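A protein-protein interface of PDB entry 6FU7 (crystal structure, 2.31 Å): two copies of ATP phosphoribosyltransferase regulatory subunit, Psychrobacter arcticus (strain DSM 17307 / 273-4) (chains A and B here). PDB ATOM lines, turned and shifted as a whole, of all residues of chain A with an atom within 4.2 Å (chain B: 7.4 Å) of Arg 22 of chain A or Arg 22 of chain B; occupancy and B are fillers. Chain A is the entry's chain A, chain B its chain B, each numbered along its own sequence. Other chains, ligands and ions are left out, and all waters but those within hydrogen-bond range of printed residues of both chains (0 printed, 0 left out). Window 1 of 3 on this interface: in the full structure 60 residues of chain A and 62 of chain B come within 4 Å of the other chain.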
ATOM      1  N   GLN A  18      13.636 -17.885  14.317  1.00  0.00           N
ATOM      2  CA  GLN A  18      12.959 -17.649  13.044  1.00  0.00           C
ATOM      3  C   GLN A  18      13.890 -17.118  11.964  1.00  0.00           C
ATOM      4  O   GLN A  18      13.814 -17.570  10.819  1.00  0.00           O
ATOM      5  CB  GLN A  18      11.802 -16.678  13.213  1.00  0.00           C
ATOM      6  CG  GLN A  18      10.880 -16.578  12.009  1.00  0.00           C
ATOM      7  CD  GLN A  18       9.922 -15.410  12.133  1.00  0.00           C
ATOM      8  OE1 GLN A  18      10.334 -14.257  12.357  1.00  0.00           O
ATOM      9  NE2 GLN A  18       8.636 -15.697  12.018  1.00  0.00           N
ATOM     10  N   GLU A  19      14.729 -16.148  12.333  1.00  0.00           N
ATOM     11  CA  GLU A  19      15.704 -15.567  11.416  1.00  0.00           C
ATOM     12  C   GLU A  19      16.763 -16.591  10.983  1.00  0.00           C
ATOM     13  O   GLU A  19      17.184 -16.608   9.818  1.00  0.00           O
ATOM     14  CB  GLU A  19      16.384 -14.341  12.069  1.00  0.00           C
ATOM     15  CG  GLU A  19      17.581 -13.772  11.318  1.00  0.00           C
ATOM     16  CD  GLU A  19      17.212 -13.168   9.977  1.00  0.00           C
ATOM     17  OE1 GLU A  19      16.248 -12.385   9.946  1.00  0.00           O
ATOM     18  OE2 GLU A  19      17.878 -13.467   8.950  1.00  0.00           O
ATOM     19  N   VAL A  20      17.220 -17.414  11.920  1.00  0.00           N
ATOM     20  CA  VAL A  20      18.167 -18.481  11.588  1.00  0.00           C
ATOM     21  C   VAL A  20      17.526 -19.505  10.623  1.00  0.00           C
ATOM     22  O   VAL A  20      18.123 -19.843   9.618  1.00  0.00           O
ATOM     23  CB  VAL A  20      18.743 -19.167  12.848  1.00  0.00           C
ATOM     24  CG1 VAL A  20      19.504 -20.438  12.490  1.00  0.00           C
ATOM     25  CG2 VAL A  20      19.678 -18.212  13.589  1.00  0.00           C
ATOM     26  N   LEU A  21      16.316 -19.958  10.926  1.00  0.00           N
ATOM     27  CA  LEU A  21      15.600 -20.887  10.043  1.00  0.00           C
ATOM     28  C   LEU A  21      15.388 -20.306   8.650  1.00  0.00           C
ATOM     29  O   LEU A  21      15.711 -20.958   7.640  1.00  0.00           O
ATOM     30  CB  LEU A  21      14.241 -21.285  10.636  1.00  0.00           C
ATOM     31  CG  LEU A  21      14.314 -22.107  11.924  1.00  0.00           C
ATOM     32  CD1 LEU A  21      12.908 -22.455  12.376  1.00  0.00           C
ATOM     33  CD2 LEU A  21      15.152 -23.334  11.773  1.00  0.00           C
ATOM     34  N   ARG A  22      14.866 -19.079   8.587  1.00  0.00           N
ATOM     35  CA  ARG A  22      14.616 -18.441   7.294  1.00  0.00           C
ATOM     36  C   ARG A  22      15.903 -18.416   6.472  1.00  0.00           C
ATOM     37  O   ARG A  22      15.913 -18.821   5.302  1.00  0.00           O
ATOM     38  CB  ARG A  22      14.073 -17.033   7.472  1.00  0.00           C
ATOM     39  CG  ARG A  22      13.648 -16.361   6.183  1.00  0.00           C
ATOM     40  CD  ARG A  22      13.513 -14.875   6.382  1.00  0.00           C
ATOM     41  NE  ARG A  22      13.270 -14.259   5.085  1.00  0.00           N
ATOM     42  CZ  ARG A  22      12.680 -13.081   4.882  1.00  0.00           C
ATOM     43  NH1 ARG A  22      12.280 -12.306   5.904  1.00  0.00           N
ATOM     44  NH2 ARG A  22      12.502 -12.644   3.622  1.00  0.00           N
ATOM     45  N   HIS A  23      16.991 -17.971   7.097  1.00  0.00           N
ATOM     46  CA  HIS A  23      18.272 -17.841   6.411  1.00  0.00           C
ATOM     47  C   HIS A  23      18.874 -19.180   5.998  1.00  0.00           C
ATOM     48  O   HIS A  23      19.342 -19.297   4.885  1.00  0.00           O
ATOM     49  CB  HIS A  23      19.295 -17.091   7.269  1.00  0.00           C
ATOM     50  CG  HIS A  23      20.535 -16.732   6.529  1.00  0.00           C
ATOM     51  ND1 HIS A  23      20.531 -15.820   5.493  1.00  0.00           N
ATOM     52  CD2 HIS A  23      21.807 -17.184   6.638  1.00  0.00           C
ATOM     53  CE1 HIS A  23      21.759 -15.702   5.013  1.00  0.00           C
ATOM     54  NE2 HIS A  23      22.553 -16.516   5.691  1.00  0.00           N
ATOM     55  N   GLN A  24      18.884 -20.164   6.890  1.00  0.00           N
ATOM     56  CA  GLN A  24      19.507 -21.456   6.598  1.00  0.00           C
ATOM     57  C   GLN A  24      18.736 -22.249   5.520  1.00  0.00           C
ATOM     58  O   GLN A  24      19.350 -22.849   4.651  1.00  0.00           O
ATOM     59  CB  GLN A  24      19.643 -22.292   7.864  1.00  0.00           C
ATOM     60  CG  GLN A  24      20.579 -21.685   8.911  1.00  0.00           C
ATOM     61  CD  GLN A  24      22.046 -21.836   8.584  1.00  0.00           C
ATOM     62  OE1 GLN A  24      22.757 -20.846   8.393  1.00  0.00           O
ATOM     63  NE2 GLN A  24      22.512 -23.083   8.524  1.00  0.00           N
ATOM     64  N   LEU A  25      17.407 -22.224   5.580  1.00  0.00           N
ATOM     65  CA  LEU A  25      16.569 -22.883   4.582  1.00  0.00           C
ATOM     66  C   LEU A  25      16.705 -22.241   3.190  1.00  0.00           C
ATOM     67  O   LEU A  25      16.768 -22.946   2.184  1.00  0.00           O
ATOM     68  CB  LEU A  25      15.107 -22.897   5.021  1.00  0.00           C
ATOM     69  CG  LEU A  25      14.880 -23.748   6.270  1.00  0.00           C
ATOM     70  CD1 LEU A  25      13.471 -23.537   6.804  1.00  0.00           C
ATOM     71  CD2 LEU A  25      15.138 -25.233   5.988  1.00  0.00           C
ATOM     72  N   THR A  26      16.772 -20.915   3.166  1.00  0.00           N
ATOM     73  CA  THR A  26      16.977 -20.149   1.942  1.00  0.00           C
ATOM     74  C   THR A  26      18.315 -20.469   1.336  1.00  0.00           C
ATOM     75  O   THR A  26      18.387 -20.772   0.143  1.00  0.00           O
ATOM     76  CB  THR A  26      16.895 -18.626   2.241  1.00  0.00           C
ATOM     77  OG1 THR A  26      15.558 -18.302   2.595  1.00  0.00           O
ATOM     78  CG2 THR A  26      17.262 -17.786   1.059  1.00  0.00           C
ATOM     79  N   ALA A 100      11.209 -16.446   0.195  1.00  0.00           N
ATOM     80  CA  ALA A 100      10.780 -16.448   1.567  1.00  0.00           C
ATOM     81  C   ALA A 100      10.328 -15.022   1.883  1.00  0.00           C
ATOM     82  O   ALA A 100      11.120 -14.089   1.792  1.00  0.00           O
ATOM     83  CB  ALA A 100      11.918 -16.905   2.488  1.00  0.00           C
ATOM     84  N   LEU A 120       7.788 -19.655   2.952  1.00  0.00           N
ATOM     85  CA  LEU A 120       9.018 -20.051   2.267  1.00  0.00           C
ATOM     86  C   LEU A 120       8.716 -21.159   1.264  1.00  0.00           C
ATOM     87  O   LEU A 120       7.953 -22.071   1.566  1.00  0.00           O
ATOM     88  CB  LEU A 120      10.039 -20.536   3.284  1.00  0.00           C
ATOM     89  CG  LEU A 120      11.431 -20.913   2.739  1.00  0.00           C
ATOM     90  CD1 LEU A 120      12.468 -20.458   3.752  1.00  0.00           C
ATOM     91  CD2 LEU A 120      11.593 -22.417   2.447  1.00  0.00           C
ATOM     92  N   VAL A 312       7.352 -20.855   7.789  1.00  0.00           N
ATOM     93  CA  VAL A 312       8.551 -20.982   8.628  1.00  0.00           C
ATOM     94  C   VAL A 312       8.220 -20.802  10.117  1.00  0.00           C
ATOM     95  O   VAL A 312       8.844 -21.460  10.965  1.00  0.00           O
ATOM     96  CB  VAL A 312       9.657 -19.976   8.229  1.00  0.00           C
ATOM     97  CG1 VAL A 312      10.888 -20.074   9.155  1.00  0.00           C
ATOM     98  CG2 VAL A 312      10.059 -20.161   6.773  1.00  0.00           C
ATOM     99  N   ALA B  15      18.626 -10.154  -4.823  1.00  0.00           N
ATOM    100  CA  ALA B  15      17.836 -10.809  -3.767  1.00  0.00           C
ATOM    101  C   ALA B  15      18.760 -11.550  -2.798  1.00  0.00           C
ATOM    102  O   ALA B  15      18.569 -11.499  -1.597  1.00  0.00           O
ATOM    103  CB  ALA B  15      16.816 -11.771  -4.354  1.00  0.00           C
ATOM    104  N   HIS B  16      19.751 -12.246  -3.332  1.00  0.00           N
ATOM    105  CA  HIS B  16      20.704 -12.939  -2.488  1.00  0.00           C
ATOM    106  C   HIS B  16      21.478 -11.933  -1.628  1.00  0.00           C
ATOM    107  O   HIS B  16      21.710 -12.152  -0.440  1.00  0.00           O
ATOM    108  CB  HIS B  16      21.655 -13.808  -3.337  1.00  0.00           C
ATOM    109  CG  HIS B  16      22.704 -14.506  -2.534  1.00  0.00           C
ATOM    110  ND1 HIS B  16      24.053 -14.277  -2.720  1.00  0.00           N
ATOM    111  CD2 HIS B  16      22.610 -15.407  -1.523  1.00  0.00           C
ATOM    112  CE1 HIS B  16      24.746 -15.017  -1.868  1.00  0.00           C
ATOM    113  NE2 HIS B  16      23.894 -15.717  -1.135  1.00  0.00           N
ATOM    114  N   LYS B  17      21.881 -10.831  -2.234  1.00  0.00           N
ATOM    115  CA  LYS B  17      22.609  -9.790  -1.503  1.00  0.00           C
ATOM    116  C   LYS B  17      21.743  -9.208  -0.373  1.00  0.00           C
ATOM    117  O   LYS B  17      22.195  -9.098   0.766  1.00  0.00           O
ATOM    118  CB  LYS B  17      23.075  -8.697  -2.449  1.00  0.00           C
ATOM    119  CG  LYS B  17      24.143  -7.810  -1.840  1.00  0.00           C
ATOM    120  CD  LYS B  17      24.272  -6.514  -2.597  1.00  0.00           C
ATOM    121  CE  LYS B  17      24.976  -6.675  -3.916  1.00  0.00           C
ATOM    122  NZ  LYS B  17      24.632  -5.538  -4.796  1.00  0.00           N
ATOM    123  N   GLN B  18      20.492  -8.886  -0.697  1.00  0.00           N
ATOM    124  CA  GLN B  18      19.543  -8.394   0.294  1.00  0.00           C
ATOM    125  C   GLN B  18      19.373  -9.351   1.480  1.00  0.00           C
ATOM    126  O   GLN B  18      19.299  -8.917   2.617  1.00  0.00           O
ATOM    127  CB  GLN B  18      18.175  -8.150  -0.326  1.00  0.00           C
ATOM    128  CG  GLN B  18      17.247  -7.342   0.582  1.00  0.00           C
ATOM    129  CD  GLN B  18      15.842  -7.258   0.042  1.00  0.00           C
ATOM    130  OE1 GLN B  18      15.198  -8.294  -0.169  1.00  0.00           O
ATOM    131  NE2 GLN B  18      15.369  -6.042  -0.215  1.00  0.00           N
ATOM    132  N   GLU B  19      19.259 -10.634   1.194  1.00  0.00           N
ATOM    133  CA  GLU B  19      19.141 -11.689   2.223  1.00  0.00           C
ATOM    134  C   GLU B  19      20.405 -11.780   3.081  1.00  0.00           C
ATOM    135  O   GLU B  19      20.309 -11.968   4.305  1.00  0.00           O
ATOM    136  CB  GLU B  19      18.836 -13.041   1.539  1.00  0.00           C
ATOM    137  CG  GLU B  19      18.975 -14.283   2.408  1.00  0.00           C
ATOM    138  CD  GLU B  19      17.938 -14.360   3.490  1.00  0.00           C
ATOM    139  OE1 GLU B  19      16.752 -14.161   3.164  1.00  0.00           O
ATOM    140  OE2 GLU B  19      18.291 -14.627   4.665  1.00  0.00           O
ATOM    141  N   VAL B  20      21.572 -11.670   2.447  1.00  0.00           N
ATOM    142  CA  VAL B  20      22.833 -11.659   3.185  1.00  0.00           C
ATOM    143  C   VAL B  20      22.914 -10.406   4.093  1.00  0.00           C
ATOM    144  O   VAL B  20      23.234 -10.524   5.261  1.00  0.00           O
ATOM    145  CB  VAL B  20      24.064 -11.753   2.245  1.00  0.00           C
ATOM    146  CG1 VAL B  20      25.361 -11.427   2.976  1.00  0.00           C
ATOM    147  CG2 VAL B  20      24.156 -13.144   1.614  1.00  0.00           C
ATOM    148  N   LEU B  21      22.613  -9.227   3.553  1.00  0.00           N
ATOM    149  CA  LEU B  21      22.620  -7.992   4.333  1.00  0.00           C
ATOM    150  C   LEU B  21      21.648  -8.065   5.518  1.00  0.00           C
ATOM    151  O   LEU B  21      22.038  -7.781   6.663  1.00  0.00           O
ATOM    152  CB  LEU B  21      22.271  -6.781   3.465  1.00  0.00           C
ATOM    153  CG  LEU B  21      23.294  -6.415   2.396  1.00  0.00           C
ATOM    154  CD1 LEU B  21      22.907  -5.176   1.623  1.00  0.00           C
ATOM    155  CD2 LEU B  21      24.668  -6.217   2.995  1.00  0.00           C
ATOM    156  N   ARG B  22      20.404  -8.468   5.246  1.00  0.00           N
ATOM    157  CA  ARG B  22      19.406  -8.557   6.304  1.00  0.00           C
ATOM    158  C   ARG B  22      19.922  -9.457   7.437  1.00  0.00           C
ATOM    159  O   ARG B  22      19.901  -9.070   8.615  1.00  0.00           O
ATOM    160  CB  ARG B  22      18.073  -9.088   5.794  1.00  0.00           C
ATOM    161  CG  ARG B  22      16.962  -8.868   6.824  1.00  0.00           C
ATOM    162  CD  ARG B  22      15.815  -9.855   6.666  1.00  0.00           C
ATOM    163  NE  ARG B  22      16.191 -11.245   6.964  1.00  0.00           N
ATOM    164  CZ  ARG B  22      16.286 -12.252   6.069  1.00  0.00           C
ATOM    165  NH1 ARG B  22      16.046 -12.062   4.762  1.00  0.00           N
ATOM    166  NH2 ARG B  22      16.633 -13.458   6.490  1.00  0.00           N
ATOM    167  N   HIS B  23      20.420 -10.630   7.058  1.00  0.00           N
ATOM    168  CA  HIS B  23      20.905 -11.609   8.039  1.00  0.00           C
ATOM    169  C   HIS B  23      22.140 -11.140   8.814  1.00  0.00           C
ATOM    170  O   HIS B  23      22.178 -11.273  10.024  1.00  0.00           O
ATOM    171  CB  HIS B  23      21.213 -12.963   7.403  1.00  0.00           C
ATOM    172  CG  HIS B  23      21.443 -14.037   8.418  1.00  0.00           C
ATOM    173  ND1 HIS B  23      20.448 -14.486   9.264  1.00  0.00           N
ATOM    174  CD2 HIS B  23      22.564 -14.719   8.758  1.00  0.00           C
ATOM    175  CE1 HIS B  23      20.948 -15.405  10.074  1.00  0.00           C
ATOM    176  NE2 HIS B  23      22.224 -15.574   9.781  1.00  0.00           N
ATOM    177  N   GLN B  24      23.138 -10.627   8.103  1.00  0.00           N
ATOM    178  CA  GLN B  24      24.404 -10.243   8.728  1.00  0.00           C
ATOM    179  C   GLN B  24      24.264  -9.022   9.646  1.00  0.00           C
ATOM    180  O   GLN B  24      24.849  -8.997  10.724  1.00  0.00           O
ATOM    181  CB  GLN B  24      25.483  -9.991   7.680  1.00  0.00           C
ATOM    182  CG  GLN B  24      25.858 -11.251   6.887  1.00  0.00           C
ATOM    183  CD  GLN B  24      26.765 -12.185   7.670  1.00  0.00           C
ATOM    184  OE1 GLN B  24      26.398 -13.326   7.974  1.00  0.00           O
ATOM    185  NE2 GLN B  24      27.963 -11.704   8.008  1.00  0.00           N
ATOM    186  N   LEU B  25      23.470  -8.043   9.225  1.00  0.00           N
ATOM    187  CA  LEU B  25      23.231  -6.841  10.042  1.00  0.00           C
ATOM    188  C   LEU B  25      22.427  -7.168  11.289  1.00  0.00           C
ATOM    189  O   LEU B  25      22.696  -6.634  12.338  1.00  0.00           O
ATOM    190  CB  LEU B  25      22.523  -5.759   9.210  1.00  0.00           C
ATOM    191  CG  LEU B  25      23.386  -5.228   8.079  1.00  0.00           C
ATOM    192  CD1 LEU B  25      22.556  -4.331   7.177  1.00  0.00           C
ATOM    193  CD2 LEU B  25      24.608  -4.494   8.602  1.00  0.00           C
ATOM    194  N   THR B  26      21.440  -8.051  11.154  1.00  0.00           N
ATOM    195  CA  THR B  26      20.635  -8.521  12.280  1.00  0.00           C
ATOM    196  C   THR B  26      21.509  -9.251  13.275  1.00  0.00           C
ATOM    197  O   THR B  26      21.444  -8.950  14.474  1.00  0.00           O
ATOM    198  CB  THR B  26      19.527  -9.461  11.775  1.00  0.00           C
ATOM    199  OG1 THR B  26      18.595  -8.685  11.024  1.00  0.00           O
ATOM    200  CG2 THR B  26      18.795 -10.161  12.900  1.00  0.00           C
ATOM    201  N   GLN B  27      22.314 -10.212  12.790  1.00  0.00           N
ATOM    202  CA  GLN B  27      23.238 -10.932  13.674  1.00  0.00           C
ATOM    203  C   GLN B  27      24.206 -10.007  14.418  1.00  0.00           C
ATOM    204  O   GLN B  27      24.469 -10.231  15.585  1.00  0.00           O
ATOM    205  CB  GLN B  27      24.060 -12.022  12.937  1.00  0.00           C
ATOM    206  CG  GLN B  27      23.308 -13.283  12.480  1.00  0.00           C
ATOM    207  CD  GLN B  27      22.216 -13.752  13.431  1.00  0.00           C
ATOM    208  OE1 GLN B  27      22.484 -14.342  14.482  1.00  0.00           O
ATOM    209  NE2 GLN B  27      20.961 -13.446  13.070  1.00  0.00           N
ATOM    210  N   GLN B  28      24.737  -8.990  13.738  1.00  0.00           N
ATOM    211  CA  GLN B  28      25.600  -8.004  14.384  1.00  0.00           C
ATOM    212  C   GLN B  28      24.901  -7.281  15.536  1.00  0.00           C
ATOM    213  O   GLN B  28      25.471  -7.167  16.613  1.00  0.00           O
ATOM    214  CB  GLN B  28      26.080  -6.956  13.401  1.00  0.00           C
ATOM    215  CG  GLN B  28      27.231  -7.431  12.540  1.00  0.00           C
ATOM    216  CD  GLN B  28      27.746  -6.316  11.679  1.00  0.00           C
ATOM    217  OE1 GLN B  28      28.125  -5.294  12.202  1.00  0.00           O
ATOM    218  NE2 GLN B  28      27.765  -6.514  10.361  1.00  0.00           N
ATOM    219  N   LEU B  29      23.679  -6.811  15.277  1.00  0.00           N
ATOM    220  CA  LEU B  29      22.845  -6.176  16.291  1.00  0.00           C
ATOM    221  C   LEU B  29      22.649  -7.088  17.510  1.00  0.00           C
ATOM    222  O   LEU B  29      22.784  -6.631  18.670  1.00  0.00           O
ATOM    223  CB  LEU B  29      21.501  -5.733  15.707  1.00  0.00           C
ATOM    224  CG  LEU B  29      21.605  -4.515  14.774  1.00  0.00           C
ATOM    225  CD1 LEU B  29      20.324  -4.208  14.009  1.00  0.00           C
ATOM    226  CD2 LEU B  29      22.028  -3.298  15.565  1.00  0.00           C
ATOM    227  N   TYR B  99      15.300  -5.015  15.073  1.00  0.00           N
ATOM    228  CA  TYR B  99      14.281  -5.499  14.189  1.00  0.00           C
ATOM    229  C   TYR B  99      14.708  -5.296  12.757  1.00  0.00           C
ATOM    230  O   TYR B  99      15.590  -4.469  12.462  1.00  0.00           O
ATOM    231  CB  TYR B  99      12.946  -4.790  14.404  1.00  0.00           C
ATOM    232  CG  TYR B  99      13.040  -3.286  14.358  1.00  0.00           C
ATOM    233  CD1 TYR B  99      12.945  -2.587  13.165  1.00  0.00           C
ATOM    234  CD2 TYR B  99      13.257  -2.563  15.528  1.00  0.00           C
ATOM    235  CE1 TYR B  99      13.042  -1.167  13.133  1.00  0.00           C
ATOM    236  CE2 TYR B  99      13.355  -1.179  15.517  1.00  0.00           C
ATOM    237  CZ  TYR B  99      13.246  -0.490  14.329  1.00  0.00           C
ATOM    238  OH  TYR B  99      13.353   0.879  14.395  1.00  0.00           O
ATOM    239  N   ALA B 100      14.093  -6.097  11.891  1.00  0.00           N
ATOM    240  CA  ALA B 100      14.225  -5.929  10.452  1.00  0.00           C
ATOM    241  C   ALA B 100      12.982  -6.529   9.823  1.00  0.00           C
ATOM    242  O   ALA B 100      12.700  -7.719  10.008  1.00  0.00           O
ATOM    243  CB  ALA B 100      15.479  -6.603   9.948  1.00  0.00           C
ATOM    244  N   GLY B 101      12.180  -5.679   9.189  1.00  0.00           N
ATOM    245  CA  GLY B 101      10.902  -6.096   8.604  1.00  0.00           C
ATOM    246  C   GLY B 101      10.448  -5.148   7.513  1.00  0.00           C
ATOM    247  O   GLY B 101      10.892  -3.995   7.445  1.00  0.00           O
ATOM    248  N   ASP B 102       9.571  -5.657   6.654  1.00  0.00           N
ATOM    249  CA  ASP B 102       8.951  -4.881   5.593  1.00  0.00           C
ATOM    250  C   ASP B 102       7.933  -3.912   6.178  1.00  0.00           C
ATOM    251  O   ASP B 102       7.204  -4.265   7.110  1.00  0.00           O
ATOM    252  CB  ASP B 102       8.242  -5.813   4.594  1.00  0.00           C
ATOM    253  CG  ASP B 102       9.204  -6.596   3.731  1.00  0.00           C
ATOM    254  OD1 ASP B 102      10.136  -7.219   4.248  1.00  0.00           O
ATOM    255  OD2 ASP B 102       9.013  -6.629   2.513  1.00  0.00           O
ATOM    256  N   LEU B 118      12.628  -2.196   3.320  1.00  0.00           N
ATOM    257  CA  LEU B 118      12.984  -3.235   4.277  1.00  0.00           C
ATOM    258  C   LEU B 118      13.649  -2.515   5.452  1.00  0.00           C
ATOM    259  O   LEU B 118      14.828  -2.187   5.428  1.00  0.00           O
ATOM    260  CB  LEU B 118      13.891  -4.281   3.627  1.00  0.00           C
ATOM    261  CG  LEU B 118      14.516  -5.364   4.504  1.00  0.00           C
ATOM    262  CD1 LEU B 118      13.551  -5.888   5.567  1.00  0.00           C
ATOM    263  CD2 LEU B 118      15.037  -6.512   3.611  1.00  0.00           C
ATOM    264  N   GLN B 119      12.842  -2.234   6.466  1.00  0.00           N
ATOM    265  CA  GLN B 119      13.222  -1.349   7.566  1.00  0.00           C
ATOM    266  C   GLN B 119      13.992  -2.136   8.615  1.00  0.00           C
ATOM    267  O   GLN B 119      13.441  -3.068   9.216  1.00  0.00           O
ATOM    268  CB  GLN B 119      11.976  -0.732   8.209  1.00  0.00           C
ATOM    269  CG  GLN B 119      12.304   0.292   9.296  1.00  0.00           C
ATOM    270  CD  GLN B 119      11.104   1.180   9.685  1.00  0.00           C
ATOM    271  OE1 GLN B 119      10.322   0.834  10.554  1.00  0.00           O
ATOM    272  NE2 GLN B 119      10.968   2.338   9.042  1.00  0.00           N
ATOM    273  N   LEU B 120      15.240  -1.737   8.857  1.00  0.00           N
ATOM    274  CA  LEU B 120      16.083  -2.350   9.889  1.00  0.00           C
ATOM    275  C   LEU B 120      16.474  -1.303  10.916  1.00  0.00           C
ATOM    276  O   LEU B 120      16.783  -0.155  10.559  1.00  0.00           O
ATOM    277  CB  LEU B 120      17.331  -2.924   9.247  1.00  0.00           C
ATOM    278  CG  LEU B 120      18.290  -3.688  10.162  1.00  0.00           C
ATOM    279  CD1 LEU B 120      18.829  -4.925   9.474  1.00  0.00           C
ATOM    280  CD2 LEU B 120      19.448  -2.797  10.572  1.00  0.00           C
ATOM    281  N   VAL B 312      17.290  -1.242   4.341  1.00  0.00           N
ATOM    282  CA  VAL B 312      18.328  -2.178   3.883  1.00  0.00           C
ATOM    283  C   VAL B 312      18.408  -2.221   2.345  1.00  0.00           C
ATOM    284  O   VAL B 312      19.484  -2.400   1.796  1.00  0.00           O
ATOM    285  CB  VAL B 312      18.089  -3.631   4.400  1.00  0.00           C
ATOM    286  CG1 VAL B 312      19.195  -4.557   3.925  1.00  0.00           C
ATOM    287  CG2 VAL B 312      18.043  -3.681   5.903  1.00  0.00           C
ATOM    288  N   LEU B 315      21.023  -0.072   0.613  1.00  0.00           N
ATOM    289  CA  LEU B 315      22.413  -0.522   0.641  1.00  0.00           C
ATOM    290  C   LEU B 315      22.841  -1.354  -0.577  1.00  0.00           C
ATOM    291  O   LEU B 315      24.048  -1.469  -0.831  1.00  0.00           O
ATOM    292  CB  LEU B 315      22.682  -1.340   1.912  1.00  0.00           C
ATOM    293  CG  LEU B 315      22.523  -0.615   3.249  1.00  0.00           C
ATOM    294  CD1 LEU B 315      22.646  -1.612   4.387  1.00  0.00           C
ATOM    295  CD2 LEU B 315      23.578   0.465   3.404  1.00  0.00           C
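A ring nitrogen (ND1) of His 23 of chain A lies within hydrogen-bond range of the side-chain carboxylate of Glu 19 of chain B, at 2.7 Å.
NH2 of Arg 22 of chain B lies within salt-bridge range of OE2 of Glu 19 of chain A, at 2.8 Å.
OE2 of Glu 19 of chain A sits at hydrogen-bond distance from ND1 of His 23 of chain B, at 2.8 Å.
The guanidinium group (NE) of Arg 22 of chain A lies within salt-bridge range of the side-chain carboxylate (OE1) of Glu 19 of chain B (3.98 Å).
Printed residues of chain B within 4 Å of Glu 19 of chain A: Arg 22 (2.8 Å), His 23 (2.8 Å) and Gln 27 (3.8 Å).
Leu 21 of chain A touches none of the printed residues of chain B.
Of chain B, only Glu 19 and Arg 22 come within 4 Å of Arg 22 of chain A.
Of the printed residues of chain B, His 23 of chain A touches Glu 19 (2.7 Å) and His 23 (3.3 Å).
Printed residues of chain A within 4 Å of Glu 19 of chain B: Arg 22 and His 23.
Leu 25 of chain B touches none of the printed residues of chain A.
Printed residues of chain A within 4 Å of Gln 27 of chain B: Glu 19.
The nearest printed residue of chain A that does not touch Arg 22 of chain B is His 23 of chain A (4.6 Å).
The nearest printed residue of chain B that does not touch Glu 19 of chain A is Thr 26 of chain B (4.1 Å).
Among the printed residues, merely in contact across the chains: His 23 of chain A with His 23 of chain B (3.3 Å), Arg 22 of chain A with Arg 22 of chain B (3.4 Å) and Glu 19 of chain A with Gln 27 of chain B (3.8 Å).
Glu 19 of chain A touches Arg 22 of chain B, and with the chains exchanged Arg 22 of chain A touches Glu 19 of chain B.
Glu 19 of chain A touches His 23 of chain B, and with the chains exchanged His 23 of chain A touches Glu 19 of chain B.
Arg 22 of chain B touches its own counterpart, Arg 22 of chain A.
His 23 of chain A touches its own counterpart, His 23 of chain B.
Of the 7 pairs that touch across the chains among the printed residues, 6 have their exchanged pair printed and touching as well.
O of Arg 22 of chain B is in hydrogen-bond range of OG1 of Thr 26 of chain B (2.8 Å).
The guanidinium group (NH2) of Arg 22 of chain A sits at hydrogen-bond distance from the backbone carbonyl oxygen (O) of Ala 100 of chain A (2.7 Å).
The guanidinium group (NH2) of Arg 22 of chain B is in salt-bridge range of the side-chain carboxylate (OE2) of Glu 19 of chain B (2.7 Å).
The side-chain hydroxyl (OG1) of Thr 26 of chain A is in hydrogen-bond range of the backbone carbonyl oxygen (O) of Arg 22 of chain A, at 2.8 Å.
Hydrophobic or aromatic side chains of chain B that line the printed part of chain A: His 23.
Along chain B the printed residues that touch a printed residue of chain A span positions 19 to 27.
Of the 12 printed residues of chain A, 3 touch a printed residue of chain B.
Hydrophobic or aromatic side chains of chain A within 4 Å of the printed part of chain B: His 23.
Among the printed residues, 7 pairs touch across the chains.
Among the printed residues, Asp or Glu carboxylates within 4 Å of a Lys or Arg side-chain nitrogen of the other chain: Glu 19 of chain A with Arg 22 of chain B and Arg 22 of chain A with Glu 19 of chain B.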
